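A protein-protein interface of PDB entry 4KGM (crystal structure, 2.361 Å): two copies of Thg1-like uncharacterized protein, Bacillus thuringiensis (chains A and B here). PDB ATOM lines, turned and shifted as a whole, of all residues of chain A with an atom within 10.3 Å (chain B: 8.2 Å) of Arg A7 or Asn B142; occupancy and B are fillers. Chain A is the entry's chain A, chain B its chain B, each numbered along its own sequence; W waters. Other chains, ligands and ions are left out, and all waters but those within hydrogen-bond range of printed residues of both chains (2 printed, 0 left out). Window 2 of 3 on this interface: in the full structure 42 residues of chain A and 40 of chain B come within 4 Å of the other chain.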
ATOM      1  N   SER A   3      -0.908  -0.021   4.303  1.00  0.00           N
ATOM      2  CA  SER A   3      -0.600  -0.810   5.490  1.00  0.00           C
ATOM      3  C   SER A   3      -1.602  -1.944   5.681  1.00  0.00           C
ATOM      4  O   SER A   3      -2.387  -2.258   4.784  1.00  0.00           O
ATOM      5  CB  SER A   3      -0.585   0.079   6.735  1.00  0.00           C
ATOM      6  OG  SER A   3      -1.866   0.635   6.976  1.00  0.00           O
ATOM      7  N   ILE A   4      -1.570  -2.553   6.859  1.00  0.00           N
ATOM      8  CA  ILE A   4      -2.493  -3.627   7.189  1.00  0.00           C
ATOM      9  C   ILE A   4      -3.853  -3.052   7.590  1.00  0.00           C
ATOM     10  O   ILE A   4      -4.900  -3.608   7.252  1.00  0.00           O
ATOM     11  CB  ILE A   4      -1.923  -4.533   8.305  1.00  0.00           C
ATOM     12  CG1 ILE A   4      -2.969  -5.546   8.775  1.00  0.00           C
ATOM     13  CG2 ILE A   4      -1.416  -3.697   9.475  1.00  0.00           C
ATOM     14  CD1 ILE A   4      -2.443  -6.518   9.807  1.00  0.00           C
ATOM     15  N   GLY A   5      -3.828  -1.923   8.291  1.00  0.00           N
ATOM     16  CA  GLY A   5      -5.044  -1.262   8.723  1.00  0.00           C
ATOM     17  C   GLY A   5      -5.849  -0.733   7.555  1.00  0.00           C
ATOM     18  O   GLY A   5      -7.079  -0.761   7.575  1.00  0.00           O
ATOM     19  N   ASP A   6      -5.151  -0.246   6.534  1.00  0.00           N
ATOM     20  CA  ASP A   6      -5.800   0.233   5.319  1.00  0.00           C
ATOM     21  C   ASP A   6      -6.493  -0.925   4.622  1.00  0.00           C
ATOM     22  O   ASP A   6      -7.620  -0.794   4.146  1.00  0.00           O
ATOM     23  CB  ASP A   6      -4.776   0.863   4.374  1.00  0.00           C
ATOM     24  CG  ASP A   6      -4.103   2.080   4.971  1.00  0.00           C
ATOM     25  OD1 ASP A   6      -4.751   2.786   5.774  1.00  0.00           O
ATOM     26  OD2 ASP A   6      -2.926   2.331   4.635  1.00  0.00           O
ATOM     27  N   ARG A   7      -5.803  -2.058   4.570  1.00  0.00           N
ATOM     28  CA  ARG A   7      -6.339  -3.260   3.953  1.00  0.00           C
ATOM     29  C   ARG A   7      -7.543  -3.752   4.744  1.00  0.00           C
ATOM     30  O   ARG A   7      -8.565  -4.124   4.170  1.00  0.00           O
ATOM     31  CB  ARG A   7      -5.258  -4.344   3.879  1.00  0.00           C
ATOM     32  CG  ARG A   7      -5.052  -4.918   2.487  1.00  0.00           C
ATOM     33  CD  ARG A   7      -3.778  -5.747   2.385  1.00  0.00           C
ATOM     34  NE  ARG A   7      -3.729  -6.822   3.372  1.00  0.00           N
ATOM     35  CZ  ARG A   7      -2.864  -6.869   4.382  1.00  0.00           C
ATOM     36  NH1 ARG A   7      -1.969  -5.904   4.537  1.00  0.00           N
ATOM     37  NH2 ARG A   7      -2.891  -7.885   5.234  1.00  0.00           N
ATOM     38  N   MET A   8      -7.423  -3.730   6.067  1.00  0.00           N
ATOM     39  CA  MET A   8      -8.507  -4.159   6.940  1.00  0.00           C
ATOM     40  C   MET A   8      -9.708  -3.225   6.858  1.00  0.00           C
ATOM     41  O   MET A   8     -10.855  -3.665   6.951  1.00  0.00           O
ATOM     42  CB  MET A   8      -8.017  -4.273   8.383  1.00  0.00           C
ATOM     43  CG  MET A   8      -7.096  -5.451   8.608  1.00  0.00           C
ATOM     44  SD  MET A   8      -7.904  -6.997   8.157  1.00  0.00           S
ATOM     45  CE  MET A   8      -6.487  -7.997   7.713  1.00  0.00           C
ATOM     46  N   LYS A   9      -9.438  -1.937   6.682  1.00  0.00           N
ATOM     47  CA  LYS A   9     -10.502  -0.949   6.576  1.00  0.00           C
ATOM     48  C   LYS A   9     -11.370  -1.188   5.343  1.00  0.00           C
ATOM     49  O   LYS A   9     -12.571  -0.929   5.368  1.00  0.00           O
ATOM     50  CB  LYS A   9      -9.925   0.468   6.550  1.00  0.00           C
ATOM     51  N   ARG A  10     -10.764  -1.686   4.270  1.00  0.00           N
ATOM     52  CA  ARG A  10     -11.501  -1.937   3.034  1.00  0.00           C
ATOM     53  C   ARG A  10     -12.383  -3.183   3.118  1.00  0.00           C
ATOM     54  O   ARG A  10     -13.467  -3.221   2.535  1.00  0.00           O
ATOM     55  CB  ARG A  10     -10.556  -2.030   1.833  1.00  0.00           C
ATOM     56  CG  ARG A  10      -9.862  -0.721   1.489  1.00  0.00           C
ATOM     57  CD  ARG A  10      -9.351  -0.723   0.057  1.00  0.00           C
ATOM     58  NE  ARG A  10      -8.441  -1.833  -0.204  1.00  0.00           N
ATOM     59  CZ  ARG A  10      -7.130  -1.787   0.006  1.00  0.00           C
ATOM     60  NH1 ARG A  10      -6.569  -0.683   0.484  1.00  0.00           N
ATOM     61  NH2 ARG A  10      -6.379  -2.848  -0.261  1.00  0.00           N
ATOM     62  N   TYR A  11     -11.915  -4.199   3.837  1.00  0.00           N
ATOM     63  CA  TYR A  11     -12.714  -5.399   4.038  1.00  0.00           C
ATOM     64  C   TYR A  11     -13.977  -5.051   4.808  1.00  0.00           C
ATOM     65  O   TYR A  11     -15.066  -5.527   4.483  1.00  0.00           O
ATOM     66  CB  TYR A  11     -11.928  -6.465   4.795  1.00  0.00           C
ATOM     67  CG  TYR A  11     -10.831  -7.120   3.991  1.00  0.00           C
ATOM     68  CD1 TYR A  11     -11.120  -7.819   2.827  1.00  0.00           C
ATOM     69  CD2 TYR A  11      -9.509  -7.059   4.409  1.00  0.00           C
ATOM     70  CE1 TYR A  11     -10.116  -8.426   2.093  1.00  0.00           C
ATOM     71  CE2 TYR A  11      -8.501  -7.659   3.682  1.00  0.00           C
ATOM     72  CZ  TYR A  11      -8.811  -8.341   2.526  1.00  0.00           C
ATOM     73  OH  TYR A  11      -7.807  -8.941   1.804  1.00  0.00           O
ATOM     74  N   GLU A  12     -13.822  -4.210   5.824  1.00  0.00           N
ATOM     75  CA  GLU A  12     -14.948  -3.792   6.643  1.00  0.00           C
ATOM     76  C   GLU A  12     -15.901  -2.911   5.842  1.00  0.00           C
ATOM     77  O   GLU A  12     -17.119  -3.032   5.962  1.00  0.00           O
ATOM     78  CB  GLU A  12     -14.463  -3.053   7.894  1.00  0.00           C
ATOM     79  CG  GLU A  12     -15.582  -2.679   8.858  1.00  0.00           C
ATOM     80  CD  GLU A  12     -15.101  -1.853  10.039  1.00  0.00           C
ATOM     81  OE1 GLU A  12     -14.038  -2.177  10.606  1.00  0.00           O
ATOM     82  OE2 GLU A  12     -15.788  -0.873  10.397  1.00  0.00           O
ATOM     83  N   ASN A  13     -15.338  -2.026   5.023  1.00  0.00           N
ATOM     84  CA  ASN A  13     -16.141  -1.099   4.232  1.00  0.00           C
ATOM     85  C   ASN A  13     -16.925  -1.775   3.113  1.00  0.00           C
ATOM     86  O   ASN A  13     -17.851  -1.188   2.554  1.00  0.00           O
ATOM     87  CB  ASN A  13     -15.276   0.028   3.664  1.00  0.00           C
ATOM     88  CG  ASN A  13     -14.818   1.004   4.733  1.00  0.00           C
ATOM     89  OD1 ASN A  13     -15.392   1.065   5.821  1.00  0.00           O
ATOM     90  ND2 ASN A  13     -13.780   1.776   4.425  1.00  0.00           N
ATOM     91  N   ALA A  14     -16.556  -3.010   2.789  1.00  0.00           N
ATOM     92  CA  ALA A  14     -17.279  -3.783   1.787  1.00  0.00           C
ATOM     93  C   ALA A  14     -18.725  -4.004   2.228  1.00  0.00           C
ATOM     94  O   ALA A  14     -19.606  -4.246   1.403  1.00  0.00           O
ATOM     95  CB  ALA A  14     -16.585  -5.112   1.537  1.00  0.00           C
ATOM     96  N   GLN B 133     -18.687  -8.912   8.554  1.00  0.00           N
ATOM     97  CA  GLN B 133     -17.962  -8.840   7.298  1.00  0.00           C
ATOM     98  C   GLN B 133     -17.383 -10.205   6.984  1.00  0.00           C
ATOM     99  O   GLN B 133     -17.467 -11.126   7.794  1.00  0.00           O
ATOM    100  CB  GLN B 133     -16.827  -7.817   7.400  1.00  0.00           C
ATOM    101  CG  GLN B 133     -15.637  -8.286   8.228  1.00  0.00           C
ATOM    102  CD  GLN B 133     -14.629  -7.177   8.490  1.00  0.00           C
ATOM    103  OE1 GLN B 133     -14.921  -6.214   9.198  1.00  0.00           O
ATOM    104  NE2 GLN B 133     -13.440  -7.307   7.917  1.00  0.00           N
ATOM    105  N   LEU B 135     -13.744 -12.255   5.415  1.00  0.00           N
ATOM    106  CA  LEU B 135     -12.309 -12.127   5.209  1.00  0.00           C
ATOM    107  C   LEU B 135     -11.795 -13.357   4.486  1.00  0.00           C
ATOM    108  O   LEU B 135     -12.263 -14.468   4.740  1.00  0.00           O
ATOM    109  CB  LEU B 135     -11.577 -11.994   6.547  1.00  0.00           C
ATOM    110  CG  LEU B 135     -11.624 -10.656   7.282  1.00  0.00           C
ATOM    111  CD1 LEU B 135     -10.815 -10.742   8.560  1.00  0.00           C
ATOM    112  CD2 LEU B 135     -11.088  -9.554   6.398  1.00  0.00           C
ATOM    113  N   PRO B 136     -10.837 -13.167   3.569  1.00  0.00           N
ATOM    114  CA  PRO B 136     -10.136 -14.324   3.006  1.00  0.00           C
ATOM    115  C   PRO B 136      -9.346 -15.045   4.094  1.00  0.00           C
ATOM    116  O   PRO B 136      -9.019 -14.440   5.116  1.00  0.00           O
ATOM    117  CB  PRO B 136      -9.192 -13.703   1.967  1.00  0.00           C
ATOM    118  CG  PRO B 136      -9.155 -12.247   2.271  1.00  0.00           C
ATOM    119  CD  PRO B 136     -10.462 -11.908   2.906  1.00  0.00           C
ATOM    120  N   GLN B 137      -9.056 -16.323   3.878  1.00  0.00           N
ATOM    121  CA  GLN B 137      -8.376 -17.138   4.878  1.00  0.00           C
ATOM    122  C   GLN B 137      -7.001 -16.584   5.243  1.00  0.00           C
ATOM    123  O   GLN B 137      -6.574 -16.679   6.392  1.00  0.00           O
ATOM    124  CB  GLN B 137      -8.238 -18.580   4.387  1.00  0.00           C
ATOM    125  CG  GLN B 137      -9.551 -19.324   4.242  1.00  0.00           C
ATOM    126  CD  GLN B 137      -9.363 -20.723   3.687  1.00  0.00           C
ATOM    127  OE1 GLN B 137      -9.740 -21.710   4.319  1.00  0.00           O
ATOM    128  NE2 GLN B 137      -8.778 -20.815   2.498  1.00  0.00           N
ATOM    129  N   ASP B 138      -6.316 -16.002   4.267  1.00  0.00           N
ATOM    130  CA  ASP B 138      -4.966 -15.496   4.483  1.00  0.00           C
ATOM    131  C   ASP B 138      -4.961 -14.084   5.073  1.00  0.00           C
ATOM    132  O   ASP B 138      -3.937 -13.398   5.049  1.00  0.00           O
ATOM    133  CB  ASP B 138      -4.155 -15.541   3.182  1.00  0.00           C
ATOM    134  CG  ASP B 138      -4.639 -14.537   2.148  1.00  0.00           C
ATOM    135  OD1 ASP B 138      -5.780 -14.042   2.272  1.00  0.00           O
ATOM    136  OD2 ASP B 138      -3.882 -14.252   1.196  1.00  0.00           O
ATOM    137  N   GLU B 139      -6.105 -13.655   5.596  1.00  0.00           N
ATOM    138  CA  GLU B 139      -6.213 -12.333   6.207  1.00  0.00           C
ATOM    139  C   GLU B 139      -6.795 -12.382   7.618  1.00  0.00           C
ATOM    140  O   GLU B 139      -6.804 -11.372   8.321  1.00  0.00           O
ATOM    141  CB  GLU B 139      -7.046 -11.392   5.330  1.00  0.00           C
ATOM    142  CG  GLU B 139      -6.377 -10.976   4.026  1.00  0.00           C
ATOM    143  CD  GLU B 139      -5.384  -9.841   4.194  1.00  0.00           C
ATOM    144  OE1 GLU B 139      -4.570  -9.882   5.139  1.00  0.00           O
ATOM    145  OE2 GLU B 139      -5.419  -8.901   3.373  1.00  0.00           O
ATOM    146  N   VAL B 140      -7.276 -13.551   8.030  1.00  0.00           N
ATOM    147  CA  VAL B 140      -7.894 -13.699   9.346  1.00  0.00           C
ATOM    148  C   VAL B 140      -6.897 -13.445  10.473  1.00  0.00           C
ATOM    149  O   VAL B 140      -7.169 -12.663  11.386  1.00  0.00           O
ATOM    150  CB  VAL B 140      -8.521 -15.091   9.534  1.00  0.00           C
ATOM    151  CG1 VAL B 140      -9.165 -15.198  10.911  1.00  0.00           C
ATOM    152  CG2 VAL B 140      -9.542 -15.359   8.446  1.00  0.00           C
ATOM    153  N   ALA B 141      -5.748 -14.110  10.405  1.00  0.00           N
ATOM    154  CA  ALA B 141      -4.696 -13.912  11.393  1.00  0.00           C
ATOM    155  C   ALA B 141      -4.274 -12.448  11.416  1.00  0.00           C
ATOM    156  O   ALA B 141      -4.070 -11.869  12.482  1.00  0.00           O
ATOM    157  CB  ALA B 141      -3.503 -14.812  11.097  1.00  0.00           C
ATOM    158  N   ASN B 142      -4.167 -11.852  10.232  1.00  0.00           N
ATOM    159  CA  ASN B 142      -3.827 -10.439  10.107  1.00  0.00           C
ATOM    160  C   ASN B 142      -4.850  -9.518  10.769  1.00  0.00           C
ATOM    161  O   ASN B 142      -4.488  -8.471  11.307  1.00  0.00           O
ATOM    162  CB  ASN B 142      -3.656 -10.055   8.637  1.00  0.00           C
ATOM    163  CG  ASN B 142      -2.522 -10.802   7.969  1.00  0.00           C
ATOM    164  OD1 ASN B 142      -1.574 -11.227   8.627  1.00  0.00           O
ATOM    165  ND2 ASN B 142      -2.612 -10.963   6.655  1.00  0.00           N
ATOM    166  N   TYR B 143      -6.123  -9.904  10.727  1.00  0.00           N
ATOM    167  CA  TYR B 143      -7.170  -9.109  11.361  1.00  0.00           C
ATOM    168  C   TYR B 143      -6.939  -8.975  12.862  1.00  0.00           C
ATOM    169  O   TYR B 143      -7.050  -7.884  13.420  1.00  0.00           O
ATOM    170  CB  TYR B 143      -8.560  -9.707  11.123  1.00  0.00           C
ATOM    171  CG  TYR B 143      -9.620  -9.046  11.980  1.00  0.00           C
ATOM    172  CD1 TYR B 143     -10.183  -7.831  11.605  1.00  0.00           C
ATOM    173  CD2 TYR B 143     -10.036  -9.619  13.179  1.00  0.00           C
ATOM    174  CE1 TYR B 143     -11.138  -7.215  12.390  1.00  0.00           C
ATOM    175  CE2 TYR B 143     -10.986  -9.006  13.972  1.00  0.00           C
ATOM    176  CZ  TYR B 143     -11.535  -7.805  13.573  1.00  0.00           C
ATOM    177  OH  TYR B 143     -12.484  -7.191  14.356  1.00  0.00           O
ATOM    178  N   PHE B 144      -6.642 -10.094  13.513  1.00  0.00           N
ATOM    179  CA  PHE B 144      -6.442 -10.102  14.955  1.00  0.00           C
ATOM    180  C   PHE B 144      -5.110  -9.466  15.331  1.00  0.00           C
ATOM    181  O   PHE B 144      -4.993  -8.835  16.380  1.00  0.00           O
ATOM    182  CB  PHE B 144      -6.564 -11.522  15.514  1.00  0.00           C
ATOM    183  CG  PHE B 144      -7.952 -12.087  15.416  1.00  0.00           C
ATOM    184  CD1 PHE B 144      -8.932 -11.711  16.320  1.00  0.00           C
ATOM    185  CD2 PHE B 144      -8.281 -12.984  14.412  1.00  0.00           C
ATOM    186  CE1 PHE B 144     -10.215 -12.222  16.229  1.00  0.00           C
ATOM    187  CE2 PHE B 144      -9.559 -13.500  14.316  1.00  0.00           C
ATOM    188  CZ  PHE B 144     -10.528 -13.119  15.226  1.00  0.00           C
ATOM    189  N   ILE B 145      -4.113  -9.629  14.466  1.00  0.00           N
ATOM    190  CA  ILE B 145      -2.838  -8.941  14.624  1.00  0.00           C
ATOM    191  C   ILE B 145      -3.079  -7.436  14.594  1.00  0.00           C
ATOM    192  O   ILE B 145      -2.508  -6.684  15.386  1.00  0.00           O
ATOM    193  CB  ILE B 145      -1.851  -9.320  13.503  1.00  0.00           C
ATOM    194  CG1 ILE B 145      -1.399 -10.773  13.651  1.00  0.00           C
ATOM    195  CG2 ILE B 145      -0.642  -8.391  13.508  1.00  0.00           C
ATOM    196  CD1 ILE B 145      -0.514 -11.252  12.517  1.00  0.00           C
ATOM    197  N   TRP B 146      -3.941  -7.012  13.677  1.00  0.00           N
ATOM    198  CA  TRP B 146      -4.337  -5.614  13.565  1.00  0.00           C
ATOM    199  C   TRP B 146      -5.035  -5.145  14.839  1.00  0.00           C
ATOM    200  O   TRP B 146      -4.788  -4.040  15.319  1.00  0.00           O
ATOM    201  CB  TRP B 146      -5.245  -5.431  12.347  1.00  0.00           C
ATOM    202  CG  TRP B 146      -5.822  -4.058  12.182  1.00  0.00           C
ATOM    203  CD1 TRP B 146      -5.142  -2.875  12.180  1.00  0.00           C
ATOM    204  CD2 TRP B 146      -7.199  -3.731  11.956  1.00  0.00           C
ATOM    205  NE1 TRP B 146      -6.013  -1.830  11.986  1.00  0.00           N
ATOM    206  CE2 TRP B 146      -7.282  -2.330  11.841  1.00  0.00           C
ATOM    207  CE3 TRP B 146      -8.371  -4.487  11.846  1.00  0.00           C
ATOM    208  CZ2 TRP B 146      -8.489  -1.668  11.621  1.00  0.00           C
ATOM    209  CZ3 TRP B 146      -9.569  -3.829  11.627  1.00  0.00           C
ATOM    210  CH2 TRP B 146      -9.617  -2.433  11.519  1.00  0.00           C
ATOM    211  N   ARG B 147      -5.894  -5.998  15.392  1.00  0.00           N
ATOM    212  CA  ARG B 147      -6.626  -5.668  16.614  1.00  0.00           C
ATOM    213  C   ARG B 147      -5.722  -5.644  17.852  1.00  0.00           C
ATOM    214  O   ARG B 147      -5.938  -4.847  18.766  1.00  0.00           O
ATOM    215  CB  ARG B 147      -7.788  -6.641  16.828  1.00  0.00           C
ATOM    216  CG  ARG B 147      -8.888  -6.576  15.767  1.00  0.00           C
ATOM    217  CD  ARG B 147      -9.760  -5.336  15.922  1.00  0.00           C
ATOM    218  NE  ARG B 147      -9.201  -4.170  15.248  1.00  0.00           N
ATOM    219  CZ  ARG B 147      -9.427  -2.912  15.616  1.00  0.00           C
ATOM    220  NH1 ARG B 147     -10.196  -2.650  16.664  1.00  0.00           N
ATOM    221  NH2 ARG B 147      -8.875  -1.915  14.939  1.00  0.00           N
ATOM    222  N   GLN B 148      -4.718  -6.517  17.878  1.00  0.00           N
ATOM    223  CA  GLN B 148      -3.778  -6.570  18.996  1.00  0.00           C
ATOM    224  C   GLN B 148      -2.844  -5.365  19.005  1.00  0.00           C
ATOM    225  O   GLN B 148      -2.477  -4.863  20.065  1.00  0.00           O
ATOM    226  CB  GLN B 148      -2.955  -7.861  18.964  1.00  0.00           C
ATOM    227  CG  GLN B 148      -3.589  -9.029  19.699  1.00  0.00           C
ATOM    228  CD  GLN B 148      -2.625 -10.185  19.900  1.00  0.00           C
ATOM    229  OE1 GLN B 148      -1.727 -10.410  19.087  1.00  0.00           O
ATOM    230  NE2 GLN B 148      -2.800 -10.920  20.992  1.00  0.00           N
ATOM    231  N   GLN B 149      -2.455  -4.910  17.819  1.00  0.00           N
ATOM    232  CA  GLN B 149      -1.593  -3.740  17.702  1.00  0.00           C
ATOM    233  C   GLN B 149      -2.328  -2.486  18.161  1.00  0.00           C
ATOM    234  O   GLN B 149      -1.739  -1.598  18.774  1.00  0.00           O
ATOM    235  CB  GLN B 149      -1.088  -3.581  16.265  1.00  0.00           C
ATOM    236  CG  GLN B 149      -0.077  -4.643  15.850  1.00  0.00           C
ATOM    237  CD  GLN B 149       0.376  -4.504  14.405  1.00  0.00           C
ATOM    238  OE1 GLN B 149      -0.208  -3.749  13.627  1.00  0.00           O
ATOM    239  NE2 GLN B 149       1.424  -5.234  14.044  1.00  0.00           N
ATOM    240  N   ILE B 226      -0.035 -12.650  18.404  1.00  0.00           N
ATOM    241  CA  ILE B 226      -0.426 -13.435  17.236  1.00  0.00           C
ATOM    242  C   ILE B 226       0.531 -13.272  16.052  1.00  0.00           C
ATOM    243  O   ILE B 226       0.663 -14.171  15.223  1.00  0.00           O
ATOM    244  CB  ILE B 226      -1.888 -13.127  16.837  1.00  0.00           C
ATOM    245  CG1 ILE B 226      -2.801 -13.336  18.047  1.00  0.00           C
ATOM    246  CG2 ILE B 226      -2.346 -14.004  15.678  1.00  0.00           C
ATOM    247  CD1 ILE B 226      -4.254 -13.042  17.783  1.00  0.00           C
ATOM    248  N   SER B 227       1.226 -12.139  15.994  1.00  0.00           N
ATOM    249  CA  SER B 227       2.177 -11.890  14.911  1.00  0.00           C
ATOM    250  C   SER B 227       3.381 -12.835  14.943  1.00  0.00           C
ATOM    251  O   SER B 227       4.088 -12.975  13.945  1.00  0.00           O
ATOM    252  CB  SER B 227       2.649 -10.433  14.921  1.00  0.00           C
ATOM    253  OG  SER B 227       3.398 -10.144  16.088  1.00  0.00           O
ATOM    254  N   ARG B 230       0.999 -17.308  14.469  1.00  0.00           N
ATOM    255  CA  ARG B 230      -0.198 -17.169  13.646  1.00  0.00           C
ATOM    256  C   ARG B 230      -1.095 -18.402  13.706  1.00  0.00           C
ATOM    257  O   ARG B 230      -2.299 -18.318  13.454  1.00  0.00           O
ATOM    258  CB  ARG B 230       0.198 -16.870  12.199  1.00  0.00           C
ATOM    259  CG  ARG B 230       1.154 -15.698  12.061  1.00  0.00           C
ATOM    260  CD  ARG B 230       1.613 -15.523  10.626  1.00  0.00           C
ATOM    261  NE  ARG B 230       0.501 -15.201   9.738  1.00  0.00           N
ATOM    262  CZ  ARG B 230       0.157 -13.965   9.395  1.00  0.00           C
ATOM    263  NH1 ARG B 230       0.843 -12.931   9.862  1.00  0.00           N
ATOM    264  NH2 ARG B 230      -0.869 -13.763   8.580  1.00  0.00           N
ATOM    265  N   VAL B 233      -4.389 -18.602  15.604  1.00  0.00           N
ATOM    266  CA  VAL B 233      -5.611 -18.190  14.923  1.00  0.00           C
ATOM    267  C   VAL B 233      -5.916 -19.104  13.738  1.00  0.00           C
ATOM    268  O   VAL B 233      -7.047 -19.564  13.572  1.00  0.00           O
ATOM    269  CB  VAL B 233      -5.517 -16.728  14.435  1.00  0.00           C
ATOM    270  CG1 VAL B 233      -6.637 -16.415  13.453  1.00  0.00           C
ATOM    271  CG2 VAL B 233      -5.559 -15.777  15.616  1.00  0.00           C
ATOM    272  N   GLU B 234      -4.899 -19.379  12.928  1.00  0.00           N
ATOM    273  CA  GLU B 234      -5.082 -20.139  11.695  1.00  0.00           C
ATOM    274  C   GLU B 234      -5.533 -21.586  11.897  1.00  0.00           C
ATOM    275  O   GLU B 234      -5.968 -22.237  10.948  1.00  0.00           O
ATOM    276  CB  GLU B 234      -3.818 -20.087  10.837  1.00  0.00           C
ATOM    277  CG  GLU B 234      -3.543 -18.711  10.251  1.00  0.00           C
ATOM    278  CD  GLU B 234      -2.358 -18.702   9.308  1.00  0.00           C
ATOM    279  OE1 GLU B 234      -1.520 -19.624   9.399  1.00  0.00           O
ATOM    280  OE2 GLU B 234      -2.267 -17.777   8.474  1.00  0.00           O
ATOM    281  N   VAL B 237      -8.953 -21.492  11.040  1.00  0.00           N
ATOM    282  CA  VAL B 237      -9.201 -20.958   9.705  1.00  0.00           C
ATOM    283  C   VAL B 237      -9.075 -22.032   8.629  1.00  0.00           C
ATOM    284  O   VAL B 237      -9.967 -22.197   7.796  1.00  0.00           O
ATOM    285  CB  VAL B 237      -8.234 -19.807   9.376  1.00  0.00           C
ATOM    286  CG1 VAL B 237      -8.502 -19.272   7.979  1.00  0.00           C
ATOM    287  CG2 VAL B 237      -8.360 -18.704  10.411  1.00  0.00           C
HETATM  288  O   HOH W   1     -13.009  -4.779  10.533  1.00  0.00           O
HETATM  289  O   HOH W   2     -11.414  -5.909   8.457  1.00  0.00           O
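The guanidinium group (NH2) of Arg A7 is in salt-bridge range of the side-chain carboxylate (OE1) of Glu B139 (2.6 Å). The guanidinium group (NH2) of Arg A7 sits close to the side-chain amide nitrogen (ND2) of Asn B142 (3.4 Å). The side-chain carboxylate (OE2) of Glu B139 is in hydrogen-bond range of the side-chain hydroxyl (OH) of Tyr A11, at 2.9 Å.
OG of Ser A3 lies close to N of Gly A5 (3.5 Å). The side-chain amide oxygen (OD1) of Asn B142 lies within hydrogen-bond range of the guanidinium group (NH2) of Arg B230, 2.6 Å away. O of Asp B138 lies within hydrogen-bond range of ND2 of Asn B142 (3.2 Å). The side-chain amide nitrogen (ND2) of Asn B142 is in hydrogen-bond range of the side-chain carboxylate (OE1) of Glu B139.
CD1 of Ile A4 touches O of Asn B142, 3.2 Å away. Trp B146 touches Ile A4 (CB to CD1, 3.9 Å). NE1 of Trp B146 touches CA of Gly A5, at 3.5 Å. Glu B139 touches Met A8. Met A8 touches Asn B142. N of Tyr B143 touches CE of Met A8, 3.6 Å away. Met A8 touches Trp B146. Tyr A11 touches Leu B135. Pro B136 touches Tyr A11 (CD to CE1, 3.6 Å). Glu A12 touches Gln B133.
Arg A7 touches two residues of chain B. Asn B142 touches just these residues of chain A: Ile A4 (3.2 Å), Arg A7 (3.4 Å) and Met A8 (3.6 Å). Of chain A, only Arg A7, Met A8 and Tyr A11 come within 4 Å of Glu B139. No residue of chain A comes within 4 Å of Ile B145. Of the printed residues of chain A, Trp B146 touches Ile A4 (3.9 Å), Gly A5 (3.5 Å) and Met A8 (3.5 Å). Printed residues of chain B within 4 Å of Met A8: Glu B139 (3.4 Å), Asn B142 (3.6 Å), Tyr B143 (3.6 Å) and Trp B146 (3.5 Å). Printed residues of chain A within 4 Å of Tyr B143: Met A8 (3.6 Å). Asp B138 touches none of the printed residues of chain A. The nearest printed residue of chain B that does not touch Gly A5 is Gln B149 (6.7 Å).
Of the 22 printed residues of chain B, 7 touch a printed residue of chain A. Printed residues of chain B that touch a printed residue of chain A: Gln B133, Leu B135, Pro B136, Glu B139, Asn B142, Tyr B143 and Trp B146. Of the 12 printed residues of chain A, 6 touch a printed residue of chain B. Hydrophobic or aromatic side chains of chain A that line the printed part of chain B: Ile A4, Met A8 and Tyr A11. Among the printed residues, 14 pairs touch across the chains.
No position is printed for both chains. Of the 14 pairs that touch across the chains among the printed residues, none has its exchanged pair printed and touching as well.
Water W2 bridges the side-chain amide nitrogen (NE2) of Gln B133 (2.5 Å) and the backbone carbonyl oxygen (O) of Met A8 (2.8 Å). Water W1 lies within hydrogen-bond range of the side-chain amide oxygen (OE1) of Gln B133 (2.7 Å) and the side-chain carboxylate (OE1) of Glu A12 (2.8 Å).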
